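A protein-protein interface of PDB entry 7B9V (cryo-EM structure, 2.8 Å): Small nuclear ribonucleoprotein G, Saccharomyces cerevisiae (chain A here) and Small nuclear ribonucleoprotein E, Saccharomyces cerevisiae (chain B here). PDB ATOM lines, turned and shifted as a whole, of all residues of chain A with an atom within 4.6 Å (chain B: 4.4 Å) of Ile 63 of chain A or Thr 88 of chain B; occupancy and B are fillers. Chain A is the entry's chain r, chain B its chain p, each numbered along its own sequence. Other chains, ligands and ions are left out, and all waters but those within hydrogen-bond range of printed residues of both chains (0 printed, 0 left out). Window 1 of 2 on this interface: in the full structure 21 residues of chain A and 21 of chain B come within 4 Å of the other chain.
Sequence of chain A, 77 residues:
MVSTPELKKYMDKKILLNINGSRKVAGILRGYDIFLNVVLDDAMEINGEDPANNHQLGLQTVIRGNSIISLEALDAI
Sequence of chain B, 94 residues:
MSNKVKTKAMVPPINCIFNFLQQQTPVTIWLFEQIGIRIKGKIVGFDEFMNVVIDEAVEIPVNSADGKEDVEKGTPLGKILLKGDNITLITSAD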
ATOM      1  N   LEU A  17      12.561  -0.843  -3.661  1.00  0.00           N
ATOM      2  CA  LEU A  17      11.931   0.424  -4.011  1.00  0.00           C
ATOM      3  C   LEU A  17      13.001   1.489  -4.166  1.00  0.00           C
ATOM      4  O   LEU A  17      13.787   1.735  -3.246  1.00  0.00           O
ATOM      5  CB  LEU A  17      10.911   0.860  -2.962  1.00  0.00           C
ATOM      6  CG  LEU A  17       9.711  -0.064  -2.857  1.00  0.00           C
ATOM      7  CD1 LEU A  17       9.900  -0.882  -1.642  1.00  0.00           C
ATOM      8  CD2 LEU A  17       8.443   0.696  -2.713  1.00  0.00           C
ATOM      9  N   ILE A  19      13.522   5.432  -4.240  1.00  0.00           N
ATOM     10  CA  ILE A  19      12.843   6.418  -3.418  1.00  0.00           C
ATOM     11  C   ILE A  19      13.468   7.773  -3.745  1.00  0.00           C
ATOM     12  O   ILE A  19      14.525   7.834  -4.377  1.00  0.00           O
ATOM     13  CB  ILE A  19      12.934   5.944  -1.917  1.00  0.00           C
ATOM     14  CG1 ILE A  19      11.868   4.865  -1.643  1.00  0.00           C
ATOM     15  CG2 ILE A  19      13.063   7.018  -0.809  1.00  0.00           C
ATOM     16  CD1 ILE A  19      11.909   4.323  -0.256  1.00  0.00           C
ATOM     17  N   ARG A  23      17.936   7.418  -2.922  1.00  0.00           N
ATOM     18  CA  ARG A  23      17.781   6.375  -1.904  1.00  0.00           C
ATOM     19  C   ARG A  23      17.041   5.123  -2.388  1.00  0.00           C
ATOM     20  O   ARG A  23      16.124   5.184  -3.214  1.00  0.00           O
ATOM     21  CB  ARG A  23      17.091   7.007  -0.701  1.00  0.00           C
ATOM     22  CG  ARG A  23      17.963   8.143  -0.144  1.00  0.00           C
ATOM     23  CD  ARG A  23      17.368   8.881   1.030  1.00  0.00           C
ATOM     24  NE  ARG A  23      16.171   9.613   0.618  1.00  0.00           N
ATOM     25  CZ  ARG A  23      15.523  10.479   1.379  1.00  0.00           C
ATOM     26  NH1 ARG A  23      15.942  10.774   2.603  1.00  0.00           N
ATOM     27  NH2 ARG A  23      14.436  11.075   0.896  1.00  0.00           N
ATOM     28  N   VAL A  25      15.418   1.291  -0.713  1.00  0.00           N
ATOM     29  CA  VAL A  25      15.112   0.394   0.401  1.00  0.00           C
ATOM     30  C   VAL A  25      14.480  -0.879  -0.152  1.00  0.00           C
ATOM     31  O   VAL A  25      13.887  -0.881  -1.237  1.00  0.00           O
ATOM     32  CB  VAL A  25      14.188   0.989   1.529  1.00  0.00           C
ATOM     33  CG1 VAL A  25      14.659   2.353   2.091  1.00  0.00           C
ATOM     34  CG2 VAL A  25      12.712   1.015   1.137  1.00  0.00           C
ATOM     35  N   LEU A  36      -0.421   4.860  -3.435  1.00  0.00           N
ATOM     36  CA  LEU A  36       0.764   4.014  -3.227  1.00  0.00           C
ATOM     37  C   LEU A  36       1.590   4.366  -2.015  1.00  0.00           C
ATOM     38  O   LEU A  36       2.812   4.212  -2.078  1.00  0.00           O
ATOM     39  CB  LEU A  36       1.698   3.969  -4.435  1.00  0.00           C
ATOM     40  CG  LEU A  36       1.030   3.555  -5.715  1.00  0.00           C
ATOM     41  CD1 LEU A  36       2.089   3.467  -6.758  1.00  0.00           C
ATOM     42  CD2 LEU A  36       0.423   2.245  -5.441  1.00  0.00           C
ATOM     43  N   ASN A  37       0.953   4.733  -0.894  1.00  0.00           N
ATOM     44  CA  ASN A  37       1.678   4.522   0.348  1.00  0.00           C
ATOM     45  C   ASN A  37       1.921   3.029   0.482  1.00  0.00           C
ATOM     46  O   ASN A  37       1.033   2.224   0.233  1.00  0.00           O
ATOM     47  CB  ASN A  37       0.909   5.030   1.571  1.00  0.00           C
ATOM     48  CG  ASN A  37       0.512   6.510   1.471  1.00  0.00           C
ATOM     49  OD1 ASN A  37       1.309   7.367   1.105  1.00  0.00           O
ATOM     50  ND2 ASN A  37      -0.742   6.795   1.800  1.00  0.00           N
ATOM     51  N   VAL A  38       3.134   2.660   0.861  1.00  0.00           N
ATOM     52  CA  VAL A  38       3.506   1.258   0.943  1.00  0.00           C
ATOM     53  C   VAL A  38       3.991   0.968   2.349  1.00  0.00           C
ATOM     54  O   VAL A  38       4.872   1.667   2.862  1.00  0.00           O
ATOM     55  CB  VAL A  38       4.563   0.938  -0.138  1.00  0.00           C
ATOM     56  CG1 VAL A  38       5.536  -0.157   0.258  1.00  0.00           C
ATOM     57  CG2 VAL A  38       3.860   0.534  -1.432  1.00  0.00           C
ATOM     58  N   LEU A  40       5.863  -2.023   4.414  1.00  0.00           N
ATOM     59  CA  LEU A  40       6.693  -3.178   4.124  1.00  0.00           C
ATOM     60  C   LEU A  40       7.568  -3.531   5.317  1.00  0.00           C
ATOM     61  O   LEU A  40       7.911  -2.677   6.140  1.00  0.00           O
ATOM     62  CB  LEU A  40       7.545  -2.966   2.879  1.00  0.00           C
ATOM     63  CG  LEU A  40       8.914  -2.314   2.989  1.00  0.00           C
ATOM     64  CD1 LEU A  40       9.448  -2.340   1.641  1.00  0.00           C
ATOM     65  CD2 LEU A  40       8.820  -0.869   3.360  1.00  0.00           C
ATOM     66  N   THR A  61       7.737  -0.369   8.706  1.00  0.00           N
ATOM     67  CA  THR A  61       8.125   0.756   7.874  1.00  0.00           C
ATOM     68  C   THR A  61       7.021   1.065   6.868  1.00  0.00           C
ATOM     69  O   THR A  61       6.512   0.160   6.203  1.00  0.00           O
ATOM     70  CB  THR A  61       9.476   0.425   7.221  1.00  0.00           C
ATOM     71  OG1 THR A  61      10.504   0.542   8.210  1.00  0.00           O
ATOM     72  CG2 THR A  61       9.798   1.343   6.120  1.00  0.00           C
ATOM     73  N   VAL A  62       6.693   2.351   6.721  1.00  0.00           N
ATOM     74  CA  VAL A  62       5.694   2.831   5.772  1.00  0.00           C
ATOM     75  C   VAL A  62       6.272   3.993   4.959  1.00  0.00           C
ATOM     76  O   VAL A  62       6.956   4.867   5.496  1.00  0.00           O
ATOM     77  CB  VAL A  62       4.360   3.176   6.487  1.00  0.00           C
ATOM     78  CG1 VAL A  62       4.475   4.321   7.482  1.00  0.00           C
ATOM     79  CG2 VAL A  62       3.274   3.498   5.476  1.00  0.00           C
ATOM     80  N   ILE A  63       6.101   3.916   3.631  1.00  0.00           N
ATOM     81  CA  ILE A  63       6.663   4.859   2.659  1.00  0.00           C
ATOM     82  C   ILE A  63       5.512   5.676   2.074  1.00  0.00           C
ATOM     83  O   ILE A  63       4.492   5.119   1.689  1.00  0.00           O
ATOM     84  CB  ILE A  63       7.386   4.106   1.525  1.00  0.00           C
ATOM     85  CG1 ILE A  63       8.576   3.329   2.044  1.00  0.00           C
ATOM     86  CG2 ILE A  63       7.882   5.047   0.423  1.00  0.00           C
ATOM     87  CD1 ILE A  63       8.910   2.146   1.167  1.00  0.00           C
ATOM     88  N   ARG A  64       5.679   6.995   2.021  1.00  0.00           N
ATOM     89  CA  ARG A  64       4.715   7.912   1.407  1.00  0.00           C
ATOM     90  C   ARG A  64       4.810   7.814  -0.112  1.00  0.00           C
ATOM     91  O   ARG A  64       5.909   7.861  -0.670  1.00  0.00           O
ATOM     92  CB  ARG A  64       4.931   9.341   1.868  1.00  0.00           C
ATOM     93  CG  ARG A  64       3.731  10.213   1.519  1.00  0.00           C
ATOM     94  CD  ARG A  64       3.782  11.551   2.208  1.00  0.00           C
ATOM     95  NE  ARG A  64       2.472  12.200   2.240  1.00  0.00           N
ATOM     96  CZ  ARG A  64       2.134  13.269   1.542  1.00  0.00           C
ATOM     97  NH1 ARG A  64       2.990  13.844   0.708  1.00  0.00           N
ATOM     98  NH2 ARG A  64       0.921  13.795   1.707  1.00  0.00           N
ATOM     99  N   GLY A  65       3.663   7.622  -0.778  1.00  0.00           N
ATOM    100  CA  GLY A  65       3.650   7.239  -2.182  1.00  0.00           C
ATOM    101  C   GLY A  65       4.254   8.212  -3.158  1.00  0.00           C
ATOM    102  O   GLY A  65       4.758   7.783  -4.204  1.00  0.00           O
ATOM    103  N   SER A  67       6.937   9.622  -2.959  1.00  0.00           N
ATOM    104  CA  SER A  67       8.363   9.413  -2.896  1.00  0.00           C
ATOM    105  C   SER A  67       8.789   8.107  -3.538  1.00  0.00           C
ATOM    106  O   SER A  67       9.982   7.921  -3.748  1.00  0.00           O
ATOM    107  CB  SER A  67       8.821   9.418  -1.439  1.00  0.00           C
ATOM    108  OG  SER A  67       8.590  10.673  -0.835  1.00  0.00           O
ATOM    109  N   ILE A  68       7.859   7.210  -3.867  1.00  0.00           N
ATOM    110  CA  ILE A  68       8.235   6.031  -4.633  1.00  0.00           C
ATOM    111  C   ILE A  68       8.544   6.478  -6.055  1.00  0.00           C
ATOM    112  O   ILE A  68       7.712   7.093  -6.726  1.00  0.00           O
ATOM    113  CB  ILE A  68       7.110   4.983  -4.582  1.00  0.00           C
ATOM    114  CG1 ILE A  68       7.080   4.293  -3.220  1.00  0.00           C
ATOM    115  CG2 ILE A  68       7.264   3.951  -5.684  1.00  0.00           C
ATOM    116  CD1 ILE A  68       5.903   3.351  -3.050  1.00  0.00           C
ATOM    117  N   TRP B  30      12.030  10.008   7.638  1.00  0.00           N
ATOM    118  CA  TRP B  30      12.953  10.445   6.589  1.00  0.00           C
ATOM    119  C   TRP B  30      12.266  11.500   5.726  1.00  0.00           C
ATOM    120  O   TRP B  30      11.165  11.265   5.222  1.00  0.00           O
ATOM    121  CB  TRP B  30      13.307   9.292   5.649  1.00  0.00           C
ATOM    122  CG  TRP B  30      14.120   8.137   6.162  1.00  0.00           C
ATOM    123  CD1 TRP B  30      14.109   7.634   7.429  1.00  0.00           C
ATOM    124  CD2 TRP B  30      14.980   7.275   5.396  1.00  0.00           C
ATOM    125  NE1 TRP B  30      14.914   6.533   7.512  1.00  0.00           N
ATOM    126  CE2 TRP B  30      15.457   6.288   6.279  1.00  0.00           C
ATOM    127  CE3 TRP B  30      15.438   7.277   4.079  1.00  0.00           C
ATOM    128  CZ2 TRP B  30      16.337   5.297   5.878  1.00  0.00           C
ATOM    129  CZ3 TRP B  30      16.262   6.262   3.664  1.00  0.00           C
ATOM    130  CH2 TRP B  30      16.717   5.294   4.564  1.00  0.00           C
ATOM    131  N   LEU B  31      12.899  12.662   5.577  1.00  0.00           N
ATOM    132  CA  LEU B  31      12.336  13.803   4.866  1.00  0.00           C
ATOM    133  C   LEU B  31      12.492  13.640   3.346  1.00  0.00           C
ATOM    134  O   LEU B  31      13.179  12.746   2.864  1.00  0.00           O
ATOM    135  CB  LEU B  31      13.008  15.084   5.346  1.00  0.00           C
ATOM    136  CG  LEU B  31      12.904  15.321   6.856  1.00  0.00           C
ATOM    137  CD1 LEU B  31      13.473  16.669   7.226  1.00  0.00           C
ATOM    138  CD2 LEU B  31      11.453  15.252   7.307  1.00  0.00           C
ATOM    139  N   PHE B  32      11.817  14.523   2.589  1.00  0.00           N
ATOM    140  CA  PHE B  32      11.621  14.355   1.146  1.00  0.00           C
ATOM    141  C   PHE B  32      12.858  14.645   0.305  1.00  0.00           C
ATOM    142  O   PHE B  32      13.444  13.724  -0.268  1.00  0.00           O
ATOM    143  CB  PHE B  32      10.440  15.216   0.673  1.00  0.00           C
ATOM    144  CG  PHE B  32      10.063  14.990  -0.766  1.00  0.00           C
ATOM    145  CD1 PHE B  32       9.311  13.882  -1.112  1.00  0.00           C
ATOM    146  CD2 PHE B  32      10.386  15.917  -1.751  1.00  0.00           C
ATOM    147  CE1 PHE B  32       8.950  13.652  -2.426  1.00  0.00           C
ATOM    148  CE2 PHE B  32      10.009  15.699  -3.074  1.00  0.00           C
ATOM    149  CZ  PHE B  32       9.289  14.563  -3.403  1.00  0.00           C
ATOM    150  N   ASN B  86       6.352  16.675   3.365  1.00  0.00           N
ATOM    151  CA  ASN B  86       7.764  16.481   3.643  1.00  0.00           C
ATOM    152  C   ASN B  86       8.115  15.106   4.212  1.00  0.00           C
ATOM    153  O   ASN B  86       9.214  14.945   4.743  1.00  0.00           O
ATOM    154  CB  ASN B  86       8.210  17.597   4.574  1.00  0.00           C
ATOM    155  CG  ASN B  86       7.873  18.967   4.008  1.00  0.00           C
ATOM    156  OD1 ASN B  86       8.284  19.312   2.910  1.00  0.00           O
ATOM    157  ND2 ASN B  86       7.097  19.738   4.754  1.00  0.00           N
ATOM    158  N   ILE B  87       7.220  14.117   4.138  1.00  0.00           N
ATOM    159  CA  ILE B  87       7.478  12.788   4.686  1.00  0.00           C
ATOM    160  C   ILE B  87       7.772  11.837   3.540  1.00  0.00           C
ATOM    161  O   ILE B  87       7.050  11.820   2.539  1.00  0.00           O
ATOM    162  CB  ILE B  87       6.232  12.259   5.418  1.00  0.00           C
ATOM    163  CG1 ILE B  87       5.787  13.202   6.523  1.00  0.00           C
ATOM    164  CG2 ILE B  87       6.474  10.852   5.991  1.00  0.00           C
ATOM    165  CD1 ILE B  87       6.738  13.350   7.627  1.00  0.00           C
ATOM    166  N   THR B  88       8.871  11.082   3.654  1.00  0.00           N
ATOM    167  CA  THR B  88       9.149   9.995   2.726  1.00  0.00           C
ATOM    168  C   THR B  88       8.930   8.622   3.366  1.00  0.00           C
ATOM    169  O   THR B  88       8.172   7.812   2.833  1.00  0.00           O
ATOM    170  CB  THR B  88      10.565  10.171   2.150  1.00  0.00           C
ATOM    171  OG1 THR B  88      10.527  11.186   1.143  1.00  0.00           O
ATOM    172  CG2 THR B  88      11.049   8.911   1.525  1.00  0.00           C
ATOM    173  N   LEU B  89       9.588   8.324   4.488  1.00  0.00           N
ATOM    174  CA  LEU B  89       9.390   7.105   5.262  1.00  0.00           C
ATOM    175  C   LEU B  89       9.053   7.437   6.704  1.00  0.00           C
ATOM    176  O   LEU B  89       9.573   8.399   7.274  1.00  0.00           O
ATOM    177  CB  LEU B  89      10.646   6.212   5.201  1.00  0.00           C
ATOM    178  CG  LEU B  89      11.010   5.511   3.900  1.00  0.00           C
ATOM    179  CD1 LEU B  89      12.315   5.821   3.503  1.00  0.00           C
ATOM    180  CD2 LEU B  89      11.263   4.110   4.344  1.00  0.00           C
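The guanidinium group (NH2) of Arg 23 of chain A lies within hydrogen-bond range of the backbone carbonyl oxygen (O) of Phe 32 of chain B (3.1 Å). The side-chain hydroxyl of Thr 88 of chain B is in hydrogen-bond range of the side-chain hydroxyl of Ser 67 of chain A, 2.8 Å away. The backbone carbonyl oxygen of Leu 31 of chain B lies within hydrogen-bond range of the guanidinium group of Arg 23 of chain A (2.9 Å). The backbone NH of Arg 64 of chain A lies within hydrogen-bond range of the backbone carbonyl oxygen of Thr 88 of chain B (2.7 Å).
The backbone carbonyl oxygen of Val 38 of chain A sits at hydrogen-bond distance from the backbone NH of Ile 63 of chain A (2.7 Å). The backbone carbonyl oxygen (O) of Thr 61 of chain A sits at hydrogen-bond distance from the backbone NH (N) of Leu 40 of chain A, at 2.9 Å. O of Trp 30 of chain B lies within hydrogen-bond range of N of Thr 88 of chain B. N of Phe 32 of chain B lies within hydrogen-bond range of O of Asn 86 of chain B (3.4 Å). N of Trp 30 of chain B sits at hydrogen-bond distance from O of Leu 89 of chain B (3.0 Å).
Ile 19 of chain A touches Thr 88 of chain B. Arg 23 of chain A touches Trp 30 of chain B. Thr 88 of chain B touches Arg 23 of chain A. Thr 61 of chain A touches Leu 89 of chain B (CG2 to CD2, 3.6 Å). O of Val 62 of chain A touches CA of Leu 89 of chain B, at 3.3 Å. Ile 63 of chain A touches Thr 88 of chain B (CA to O, 3.3 Å). Leu 89 of chain B touches Ile 63 of chain A (CD2 to CG1, 3.6 Å). Arg 64 of chain A touches Ile 87 of chain B. Ser 67 of chain A touches Phe 32 of chain B (OG to CD1, 3.3 Å). Ser 67 of chain A touches Ile 87 of chain B.
Ile 63 of chain A touches just these residues of chain B: Thr 88 (3.3 Å) and Leu 89 (3.6 Å). Thr 88 of chain B touches just these residues of chain A: Ile 19, Arg 23, Ile 63, Arg 64 and Ser 67. Printed residues of chain B within 4 Å of Ile 19 of chain A: Thr 88 (3.6 Å). Printed residues of chain B within 4 Å of Arg 64 of chain A: Ile 87 and Thr 88. Asn 86 of chain B touches none of the printed residues of chain A. The nearest printed residue of chain B that does not touch Val 62 of chain A is Thr 88 of chain B (4.2 Å).
Of the 15 printed residues of chain A, 7 touch a printed residue of chain B. Hydrophobic or aromatic side chains of chain A that line the printed part of chain B: Ile 19 and Ile 63. Of the 7 printed residues of chain B, 6 touch a printed residue of chain A. Hydrophobic or aromatic side chains of chain B that line the printed part of chain A: Trp 30, Phe 32 and Leu 89. Among the printed residues, no Asp or Glu carboxylate lies within 4 Å of a Lys or Arg side-chain nitrogen of the other chain.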
